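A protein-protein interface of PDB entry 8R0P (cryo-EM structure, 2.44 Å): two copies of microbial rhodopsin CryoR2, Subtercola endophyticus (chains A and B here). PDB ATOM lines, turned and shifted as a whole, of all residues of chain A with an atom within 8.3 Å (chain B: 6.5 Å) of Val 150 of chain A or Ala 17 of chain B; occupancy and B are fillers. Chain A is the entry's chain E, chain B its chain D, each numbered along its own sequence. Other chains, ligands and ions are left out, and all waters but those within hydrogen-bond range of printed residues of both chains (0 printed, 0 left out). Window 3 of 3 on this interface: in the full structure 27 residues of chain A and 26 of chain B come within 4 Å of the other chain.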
ATOM      1  N   TRP A  10      20.317  24.472   7.959  1.00  0.00           N
ATOM      2  CA  TRP A  10      21.279  23.847   8.854  1.00  0.00           C
ATOM      3  C   TRP A  10      22.295  23.025   8.064  1.00  0.00           C
ATOM      4  O   TRP A  10      23.134  22.340   8.640  1.00  0.00           O
ATOM      5  CB  TRP A  10      20.565  22.974   9.891  1.00  0.00           C
ATOM      6  CG  TRP A  10      19.601  21.979   9.304  1.00  0.00           C
ATOM      7  CD1 TRP A  10      19.865  20.749   8.785  1.00  0.00           C
ATOM      8  CD2 TRP A  10      18.181  22.174   9.158  1.00  0.00           C
ATOM      9  NE1 TRP A  10      18.718  20.161   8.338  1.00  0.00           N
ATOM     10  CE2 TRP A  10      17.667  21.014   8.545  1.00  0.00           C
ATOM     11  CE3 TRP A  10      17.304  23.218   9.477  1.00  0.00           C
ATOM     12  CZ2 TRP A  10      16.315  20.864   8.265  1.00  0.00           C
ATOM     13  CZ3 TRP A  10      15.965  23.061   9.196  1.00  0.00           C
ATOM     14  CH2 TRP A  10      15.483  21.905   8.585  1.00  0.00           C
ATOM     15  N   ILE A  94      20.122  21.018  13.135  1.00  0.00           N
ATOM     16  CA  ILE A  94      18.699  21.099  12.881  1.00  0.00           C
ATOM     17  C   ILE A  94      17.962  21.508  14.159  1.00  0.00           C
ATOM     18  O   ILE A  94      16.834  21.978  14.088  1.00  0.00           O
ATOM     19  CB  ILE A  94      18.140  19.766  12.339  1.00  0.00           C
ATOM     20  CG1 ILE A  94      16.685  19.914  11.908  1.00  0.00           C
ATOM     21  CG2 ILE A  94      18.266  18.693  13.391  1.00  0.00           C
ATOM     22  CD1 ILE A  94      16.215  18.875  10.978  1.00  0.00           C
ATOM     23  N   SER A  98      14.696  23.728  15.267  1.00  0.00           N
ATOM     24  CA  SER A  98      13.548  23.016  15.770  1.00  0.00           C
ATOM     25  C   SER A  98      13.080  23.679  17.060  1.00  0.00           C
ATOM     26  O   SER A  98      11.880  23.844  17.285  1.00  0.00           O
ATOM     27  CB  SER A  98      13.909  21.577  15.957  1.00  0.00           C
ATOM     28  OG  SER A  98      13.646  20.887  14.745  1.00  0.00           O
ATOM     29  N   TYR A 101      10.556  26.570  16.727  1.00  0.00           N
ATOM     30  CA  TYR A 101       9.182  26.108  16.554  1.00  0.00           C
ATOM     31  C   TYR A 101       8.614  25.596  17.873  1.00  0.00           C
ATOM     32  O   TYR A 101       7.415  25.712  18.123  1.00  0.00           O
ATOM     33  CB  TYR A 101       9.077  24.959  15.558  1.00  0.00           C
ATOM     34  CG  TYR A 101       9.229  25.438  14.136  1.00  0.00           C
ATOM     35  CD1 TYR A 101       8.154  25.917  13.437  1.00  0.00           C
ATOM     36  CD2 TYR A 101      10.461  25.422  13.508  1.00  0.00           C
ATOM     37  CE1 TYR A 101       8.298  26.371  12.139  1.00  0.00           C
ATOM     38  CE2 TYR A 101      10.626  25.866  12.211  1.00  0.00           C
ATOM     39  CZ  TYR A 101       9.543  26.378  11.536  1.00  0.00           C
ATOM     40  OH  TYR A 101       9.738  26.825  10.256  1.00  0.00           O
ATOM     41  N   PHE A 142       2.545  24.133  14.237  1.00  0.00           N
ATOM     42  CA  PHE A 142       2.896  22.722  14.164  1.00  0.00           C
ATOM     43  C   PHE A 142       2.949  22.350  12.693  1.00  0.00           C
ATOM     44  O   PHE A 142       3.865  21.666  12.260  1.00  0.00           O
ATOM     45  CB  PHE A 142       1.882  21.883  14.950  1.00  0.00           C
ATOM     46  CG  PHE A 142       2.142  20.402  14.901  1.00  0.00           C
ATOM     47  CD1 PHE A 142       3.235  19.862  15.554  1.00  0.00           C
ATOM     48  CD2 PHE A 142       1.338  19.569  14.144  1.00  0.00           C
ATOM     49  CE1 PHE A 142       3.494  18.510  15.474  1.00  0.00           C
ATOM     50  CE2 PHE A 142       1.622  18.223  14.037  1.00  0.00           C
ATOM     51  CZ  PHE A 142       2.670  17.695  14.734  1.00  0.00           C
ATOM     52  N   CYS A 143       1.989  22.853  11.934  1.00  0.00           N
ATOM     53  CA  CYS A 143       2.068  22.744  10.494  1.00  0.00           C
ATOM     54  C   CYS A 143       3.385  23.266   9.945  1.00  0.00           C
ATOM     55  O   CYS A 143       3.889  22.734   8.975  1.00  0.00           O
ATOM     56  CB  CYS A 143       0.938  23.518   9.846  1.00  0.00           C
ATOM     57  SG  CYS A 143      -0.644  22.732  10.220  1.00  0.00           S
ATOM     58  N   GLY A 144       3.903  24.354  10.519  1.00  0.00           N
ATOM     59  CA  GLY A 144       5.170  24.910  10.087  1.00  0.00           C
ATOM     60  C   GLY A 144       6.269  23.914  10.333  1.00  0.00           C
ATOM     61  O   GLY A 144       6.964  23.550   9.408  1.00  0.00           O
ATOM     62  N   PHE A 145       6.323  23.417  11.560  1.00  0.00           N
ATOM     63  CA  PHE A 145       7.270  22.401  11.987  1.00  0.00           C
ATOM     64  C   PHE A 145       7.200  21.151  11.102  1.00  0.00           C
ATOM     65  O   PHE A 145       8.205  20.500  10.839  1.00  0.00           O
ATOM     66  CB  PHE A 145       6.995  22.096  13.447  1.00  0.00           C
ATOM     67  CG  PHE A 145       7.939  21.119  14.083  1.00  0.00           C
ATOM     68  CD1 PHE A 145       9.241  21.469  14.344  1.00  0.00           C
ATOM     69  CD2 PHE A 145       7.509  19.853  14.459  1.00  0.00           C
ATOM     70  CE1 PHE A 145      10.097  20.576  14.982  1.00  0.00           C
ATOM     71  CE2 PHE A 145       8.380  18.945  15.030  1.00  0.00           C
ATOM     72  CZ  PHE A 145       9.672  19.312  15.297  1.00  0.00           C
ATOM     73  N   LEU A 146       6.031  20.822  10.601  1.00  0.00           N
ATOM     74  CA  LEU A 146       5.948  19.658   9.768  1.00  0.00           C
ATOM     75  C   LEU A 146       6.718  19.936   8.489  1.00  0.00           C
ATOM     76  O   LEU A 146       7.679  19.207   8.234  1.00  0.00           O
ATOM     77  CB  LEU A 146       4.475  19.288   9.520  1.00  0.00           C
ATOM     78  CG  LEU A 146       3.734  18.650  10.714  1.00  0.00           C
ATOM     79  CD1 LEU A 146       2.338  18.239  10.296  1.00  0.00           C
ATOM     80  CD2 LEU A 146       4.466  17.444  11.303  1.00  0.00           C
ATOM     81  N   GLY A 147       6.293  20.967   7.725  1.00  0.00           N
ATOM     82  CA  GLY A 147       6.884  21.335   6.444  1.00  0.00           C
ATOM     83  C   GLY A 147       8.407  21.559   6.553  1.00  0.00           C
ATOM     84  O   GLY A 147       9.198  21.100   5.737  1.00  0.00           O
ATOM     85  N   ALA A 148       8.853  22.180   7.621  1.00  0.00           N
ATOM     86  CA  ALA A 148      10.204  22.664   7.643  1.00  0.00           C
ATOM     87  C   ALA A 148      11.177  21.665   8.236  1.00  0.00           C
ATOM     88  O   ALA A 148      12.373  21.821   8.020  1.00  0.00           O
ATOM     89  CB  ALA A 148      10.244  23.919   8.456  1.00  0.00           C
ATOM     90  N   ILE A 149      10.709  20.751   9.082  1.00  0.00           N
ATOM     91  CA  ILE A 149      11.627  19.961   9.898  1.00  0.00           C
ATOM     92  C   ILE A 149      11.358  18.472   9.775  1.00  0.00           C
ATOM     93  O   ILE A 149      12.313  17.713   9.740  1.00  0.00           O
ATOM     94  CB  ILE A 149      11.551  20.376  11.364  1.00  0.00           C
ATOM     95  CG1 ILE A 149      11.837  21.866  11.506  1.00  0.00           C
ATOM     96  CG2 ILE A 149      12.509  19.553  12.204  1.00  0.00           C
ATOM     97  CD1 ILE A 149      13.302  22.204  11.627  1.00  0.00           C
ATOM     98  N   VAL A 150      10.081  18.067   9.742  1.00  0.00           N
ATOM     99  CA  VAL A 150       9.742  16.695  10.077  1.00  0.00           C
ATOM    100  C   VAL A 150       9.663  15.906   8.780  1.00  0.00           C
ATOM    101  O   VAL A 150      10.460  14.984   8.574  1.00  0.00           O
ATOM    102  CB  VAL A 150       8.481  16.598  10.964  1.00  0.00           C
ATOM    103  CG1 VAL A 150       7.916  15.191  11.031  1.00  0.00           C
ATOM    104  CG2 VAL A 150       8.788  17.120  12.367  1.00  0.00           C
ATOM    105  N   ILE A 151       8.768  16.296   7.893  1.00  0.00           N
ATOM    106  CA  ILE A 151       8.686  15.607   6.623  1.00  0.00           C
ATOM    107  C   ILE A 151       9.972  15.734   5.804  1.00  0.00           C
ATOM    108  O   ILE A 151      10.421  16.837   5.503  1.00  0.00           O
ATOM    109  CB  ILE A 151       7.525  16.176   5.836  1.00  0.00           C
ATOM    110  CG1 ILE A 151       6.225  15.947   6.605  1.00  0.00           C
ATOM    111  CG2 ILE A 151       7.561  15.596   4.437  1.00  0.00           C
ATOM    112  CD1 ILE A 151       5.063  16.707   6.019  1.00  0.00           C
ATOM    113  N   ASP A 152      10.570  14.590   5.472  1.00  0.00           N
ATOM    114  CA  ASP A 152      11.700  14.472   4.565  1.00  0.00           C
ATOM    115  C   ASP A 152      12.917  15.203   5.113  1.00  0.00           C
ATOM    116  O   ASP A 152      13.882  15.446   4.410  1.00  0.00           O
ATOM    117  CB  ASP A 152      11.255  14.851   3.166  1.00  0.00           C
ATOM    118  CG  ASP A 152      10.192  13.900   2.637  1.00  0.00           C
ATOM    119  OD1 ASP A 152      10.036  12.816   3.225  1.00  0.00           O
ATOM    120  OD2 ASP A 152       9.512  14.245   1.639  1.00  0.00           O
ATOM    121  N   ASN A 153      12.905  15.481   6.397  1.00  0.00           N
ATOM    122  CA  ASN A 153      14.009  16.191   7.008  1.00  0.00           C
ATOM    123  C   ASN A 153      14.082  17.634   6.540  1.00  0.00           C
ATOM    124  O   ASN A 153      15.153  18.220   6.613  1.00  0.00           O
ATOM    125  CB  ASN A 153      15.350  15.537   6.709  1.00  0.00           C
ATOM    126  CG  ASN A 153      15.312  14.036   6.855  1.00  0.00           C
ATOM    127  OD1 ASN A 153      14.966  13.319   5.909  1.00  0.00           O
ATOM    128  ND2 ASN A 153      15.677  13.574   8.038  1.00  0.00           N
ATOM    129  N   GLY A 154      12.952  18.193   6.113  1.00  0.00           N
ATOM    130  CA  GLY A 154      12.905  19.566   5.669  1.00  0.00           C
ATOM    131  C   GLY A 154      13.045  19.690   4.162  1.00  0.00           C
ATOM    132  O   GLY A 154      12.856  20.769   3.607  1.00  0.00           O
ATOM    133  N   THR A 155      13.325  18.604   3.471  1.00  0.00           N
ATOM    134  CA  THR A 155      13.823  18.782   2.125  1.00  0.00           C
ATOM    135  C   THR A 155      12.749  18.605   1.081  1.00  0.00           C
ATOM    136  O   THR A 155      13.067  18.564  -0.090  1.00  0.00           O
ATOM    137  CB  THR A 155      14.948  17.803   1.846  1.00  0.00           C
ATOM    138  OG1 THR A 155      14.267  16.589   1.497  1.00  0.00           O
ATOM    139  CG2 THR A 155      15.887  17.729   3.041  1.00  0.00           C
ATOM    140  N   ASN A 156      11.491  18.489   1.461  1.00  0.00           N
ATOM    141  CA  ASN A 156      10.516  18.192   0.433  1.00  0.00           C
ATOM    142  C   ASN A 156       9.825  19.481   0.059  1.00  0.00           C
ATOM    143  O   ASN A 156       9.102  20.016   0.871  1.00  0.00           O
ATOM    144  CB  ASN A 156       9.548  17.089   0.873  1.00  0.00           C
ATOM    145  CG  ASN A 156       8.462  16.799  -0.146  1.00  0.00           C
ATOM    146  OD1 ASN A 156       8.605  17.070  -1.331  1.00  0.00           O
ATOM    147  ND2 ASN A 156       7.367  16.217   0.301  1.00  0.00           N
ATOM    148  N   ALA A 159       5.954  19.379   0.324  1.00  0.00           N
ATOM    149  CA  ALA A 159       5.538  19.365   1.705  1.00  0.00           C
ATOM    150  C   ALA A 159       5.699  20.774   2.264  1.00  0.00           C
ATOM    151  O   ALA A 159       4.747  21.365   2.744  1.00  0.00           O
ATOM    152  CB  ALA A 159       6.352  18.362   2.496  1.00  0.00           C
ATOM    153  N   TRP A 163       2.431  22.525   3.693  1.00  0.00           N
ATOM    154  CA  TRP A 163       2.242  22.753   5.100  1.00  0.00           C
ATOM    155  C   TRP A 163       2.266  24.227   5.465  1.00  0.00           C
ATOM    156  O   TRP A 163       1.564  24.628   6.375  1.00  0.00           O
ATOM    157  CB  TRP A 163       3.215  21.912   5.919  1.00  0.00           C
ATOM    158  CG  TRP A 163       2.770  20.479   5.860  1.00  0.00           C
ATOM    159  CD1 TRP A 163       3.239  19.486   5.058  1.00  0.00           C
ATOM    160  CD2 TRP A 163       1.656  19.915   6.581  1.00  0.00           C
ATOM    161  NE1 TRP A 163       2.544  18.328   5.263  1.00  0.00           N
ATOM    162  CE2 TRP A 163       1.558  18.563   6.181  1.00  0.00           C
ATOM    163  CE3 TRP A 163       0.748  20.413   7.526  1.00  0.00           C
ATOM    164  CZ2 TRP A 163       0.592  17.710   6.708  1.00  0.00           C
ATOM    165  CZ3 TRP A 163      -0.202  19.565   8.041  1.00  0.00           C
ATOM    166  CH2 TRP A 163      -0.276  18.236   7.637  1.00  0.00           C
ATOM    167  N   LEU B  14      14.219   4.671  15.948  1.00  0.00           N
ATOM    168  CA  LEU B  14      13.346   5.750  15.535  1.00  0.00           C
ATOM    169  C   LEU B  14      13.852   6.365  14.231  1.00  0.00           C
ATOM    170  O   LEU B  14      14.997   6.795  14.152  1.00  0.00           O
ATOM    171  CB  LEU B  14      13.323   6.795  16.658  1.00  0.00           C
ATOM    172  CG  LEU B  14      12.835   6.302  18.012  1.00  0.00           C
ATOM    173  CD1 LEU B  14      12.980   7.399  19.034  1.00  0.00           C
ATOM    174  CD2 LEU B  14      11.388   5.807  17.919  1.00  0.00           C
ATOM    175  N   SER B  15      12.949   6.525  13.266  1.00  0.00           N
ATOM    176  CA  SER B  15      13.191   7.418  12.148  1.00  0.00           C
ATOM    177  C   SER B  15      13.514   8.825  12.627  1.00  0.00           C
ATOM    178  O   SER B  15      13.287   9.165  13.783  1.00  0.00           O
ATOM    179  CB  SER B  15      12.028   7.447  11.204  1.00  0.00           C
ATOM    180  OG  SER B  15      11.013   8.320  11.625  1.00  0.00           O
ATOM    181  N   ASN B  16      14.013   9.647  11.699  1.00  0.00           N
ATOM    182  CA  ASN B  16      14.358  11.029  11.987  1.00  0.00           C
ATOM    183  C   ASN B  16      13.085  11.822  12.267  1.00  0.00           C
ATOM    184  O   ASN B  16      13.026  12.577  13.234  1.00  0.00           O
ATOM    185  CB  ASN B  16      15.176  11.643  10.845  1.00  0.00           C
ATOM    186  CG  ASN B  16      16.662  11.404  11.000  1.00  0.00           C
ATOM    187  OD1 ASN B  16      17.143  11.082  12.091  1.00  0.00           O
ATOM    188  ND2 ASN B  16      17.394  11.567   9.911  1.00  0.00           N
ATOM    189  N   ALA B  17      12.070  11.628  11.434  1.00  0.00           N
ATOM    190  CA  ALA B  17      10.809  12.281  11.704  1.00  0.00           C
ATOM    191  C   ALA B  17      10.394  11.991  13.140  1.00  0.00           C
ATOM    192  O   ALA B  17      10.078  12.910  13.903  1.00  0.00           O
ATOM    193  CB  ALA B  17       9.746  11.829  10.749  1.00  0.00           C
ATOM    194  N   GLU B  18      10.417  10.693  13.482  1.00  0.00           N
ATOM    195  CA  GLU B  18       9.959  10.190  14.760  1.00  0.00           C
ATOM    196  C   GLU B  18      10.781  10.812  15.868  1.00  0.00           C
ATOM    197  O   GLU B  18      10.220  11.330  16.832  1.00  0.00           O
ATOM    198  CB  GLU B  18      10.048   8.679  14.784  1.00  0.00           C
ATOM    199  CG  GLU B  18       8.914   8.052  13.986  1.00  0.00           C
ATOM    200  CD  GLU B  18       9.149   6.585  13.630  1.00  0.00           C
ATOM    201  OE1 GLU B  18       8.265   5.998  12.944  1.00  0.00           O
ATOM    202  OE2 GLU B  18      10.248   6.029  13.987  1.00  0.00           O
ATOM    203  N   HIS B  19      12.088  10.837  15.711  1.00  0.00           N
ATOM    204  CA  HIS B  19      12.896  11.364  16.795  1.00  0.00           C
ATOM    205  C   HIS B  19      12.671  12.865  16.948  1.00  0.00           C
ATOM    206  O   HIS B  19      12.907  13.433  18.015  1.00  0.00           O
ATOM    207  CB  HIS B  19      14.354  11.005  16.562  1.00  0.00           C
ATOM    208  CG  HIS B  19      15.284  11.406  17.601  1.00  0.00           C
ATOM    209  ND1 HIS B  19      15.885  12.639  17.617  1.00  0.00           N
ATOM    210  CD2 HIS B  19      15.839  10.687  18.592  1.00  0.00           C
ATOM    211  CE1 HIS B  19      16.736  12.683  18.660  1.00  0.00           C
ATOM    212  NE2 HIS B  19      16.732  11.513  19.268  1.00  0.00           N
ATOM    213  N   GLN B  20      12.220  13.505  15.869  1.00  0.00           N
ATOM    214  CA  GLN B  20      12.102  14.948  15.857  1.00  0.00           C
ATOM    215  C   GLN B  20      10.800  15.288  16.575  1.00  0.00           C
ATOM    216  O   GLN B  20      10.836  16.050  17.540  1.00  0.00           O
ATOM    217  CB  GLN B  20      12.191  15.446  14.408  1.00  0.00           C
ATOM    218  CG  GLN B  20      12.800  16.824  14.258  1.00  0.00           C
ATOM    219  CD  GLN B  20      14.184  16.903  14.824  1.00  0.00           C
ATOM    220  OE1 GLN B  20      15.010  16.046  14.544  1.00  0.00           O
ATOM    221  NE2 GLN B  20      14.448  17.905  15.642  1.00  0.00           N
ATOM    222  N   LEU B  21       9.687  14.672  16.122  1.00  0.00           N
ATOM    223  CA  LEU B  21       8.397  14.747  16.797  1.00  0.00           C
ATOM    224  C   LEU B  21       8.506  14.449  18.301  1.00  0.00           C
ATOM    225  O   LEU B  21       7.910  15.139  19.121  1.00  0.00           O
ATOM    226  CB  LEU B  21       7.459  13.759  16.147  1.00  0.00           C
ATOM    227  CG  LEU B  21       6.944  14.184  14.795  1.00  0.00           C
ATOM    228  CD1 LEU B  21       6.232  13.028  14.119  1.00  0.00           C
ATOM    229  CD2 LEU B  21       5.982  15.352  14.920  1.00  0.00           C
ATOM    230  N   ILE B  22       9.267  13.441  18.714  1.00  0.00           N
ATOM    231  CA  ILE B  22       9.261  13.148  20.133  1.00  0.00           C
ATOM    232  C   ILE B  22       9.871  14.325  20.877  1.00  0.00           C
ATOM    233  O   ILE B  22       9.357  14.742  21.906  1.00  0.00           O
ATOM    234  CB  ILE B  22       9.940  11.803  20.472  1.00  0.00           C
ATOM    235  CG1 ILE B  22       9.079  10.636  20.001  1.00  0.00           C
ATOM    236  CG2 ILE B  22      10.250  11.684  21.952  1.00  0.00           C
ATOM    237  CD1 ILE B  22       9.863   9.405  19.641  1.00  0.00           C
ATOM    238  N   TYR B  24      10.042  17.400  20.075  1.00  0.00           N
ATOM    239  CA  TYR B  24       9.121  18.503  20.028  1.00  0.00           C
ATOM    240  C   TYR B  24       8.125  18.408  21.181  1.00  0.00           C
ATOM    241  O   TYR B  24       8.144  19.259  22.075  1.00  0.00           O
ATOM    242  CB  TYR B  24       8.444  18.446  18.673  1.00  0.00           C
ATOM    243  CG  TYR B  24       7.427  19.535  18.450  1.00  0.00           C
ATOM    244  CD1 TYR B  24       7.818  20.845  18.106  1.00  0.00           C
ATOM    245  CD2 TYR B  24       6.075  19.239  18.509  1.00  0.00           C
ATOM    246  CE1 TYR B  24       6.872  21.819  17.805  1.00  0.00           C
ATOM    247  CE2 TYR B  24       5.122  20.214  18.230  1.00  0.00           C
ATOM    248  CZ  TYR B  24       5.516  21.502  17.885  1.00  0.00           C
ATOM    249  OH  TYR B  24       4.508  22.377  17.602  1.00  0.00           O
ATOM    250  N   THR B 228       6.476   5.834  19.090  1.00  0.00           N
ATOM    251  CA  THR B 228       6.371   7.285  18.980  1.00  0.00           C
ATOM    252  C   THR B 228       4.971   7.679  19.413  1.00  0.00           C
ATOM    253  O   THR B 228       4.807   8.556  20.259  1.00  0.00           O
ATOM    254  CB  THR B 228       6.749   7.765  17.569  1.00  0.00           C
ATOM    255  OG1 THR B 228       8.157   7.558  17.499  1.00  0.00           O
ATOM    256  CG2 THR B 228       6.462   9.226  17.304  1.00  0.00           C
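No position is printed for both chains.
Tyr 101 of chain A touches Tyr 24 of chain B (O to CE1, 3.9 Å).
CD1 of Phe 142 of chain A touches CE2 of Tyr 24 of chain B, 3.3 Å away.
Phe 145 of chain A touches Tyr 24 of chain B.
CG2 of Ile 149 of chain A touches CG of Gln 20 of chain B, at 3.4 Å.
CG1 of Val 150 of chain A touches CB of Ala 17 of chain B, 3.8 Å away.
Hydrophobic or aromatic side chains of chain B that line the printed part of chain A: Ala 17 and Tyr 24.
Hydrophobic or aromatic side chains of chain A that line the printed part of chain B: Phe 142, Phe 145, Ile 149 and Val 150.
Among the printed residues, 7 pairs touch across the chains.
Among the printed residues, no Asp or Glu carboxylate lies within 4 Å of a Lys or Arg side-chain nitrogen of the other chain.
Of the printed residues of chain B, Val 150 of chain A touches Ala 17 (3.8 Å).
Of chain A, only Val 150 (3.8 Å) comes within 4 Å of Ala 17 of chain B.
Of the printed residues of chain B, Phe 142 of chain A touches Tyr 24.
Of the printed residues of chain B, Tyr 101 of chain A touches Tyr 24.
Of the printed residues of chain B, Phe 145 of chain A touches Tyr 24.
Ala 148 of chain A touches none of the printed residues of chain B.
Gly 154 of chain A touches none of the printed residues of chain B.
The nearest residue of chain A that does not touch Ala 17 of chain B is Asn 153 of chain A (5.3 Å).
The nearest printed residue of chain A that does not touch Gln 20 of chain B is Phe 145 of chain A (4.1 Å).
O of Phe 145 of chain A is in hydrogen-bond range of N of Val 150 of chain A, 3.3 Å away.
The side-chain hydroxyl (OG) of Ser 15 of chain B lies close to the backbone NH (N) of Ala 17 of chain B (3.5 Å).
The backbone carbonyl oxygen (O) of Ile 94 of chain A sits at hydrogen-bond distance from the side-chain hydroxyl (OG) of Ser 98 of chain A, at 3.4 Å.
The side-chain hydroxyl of Ser 98 of chain A lies within hydrogen-bond range of the side-chain amide nitrogen of Gln 20 of chain B (3.2 Å).
The side-chain amide nitrogen of Asn 16 of chain B sits close to the side-chain amide nitrogen of Asn 153 of chain A (3.2 Å).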
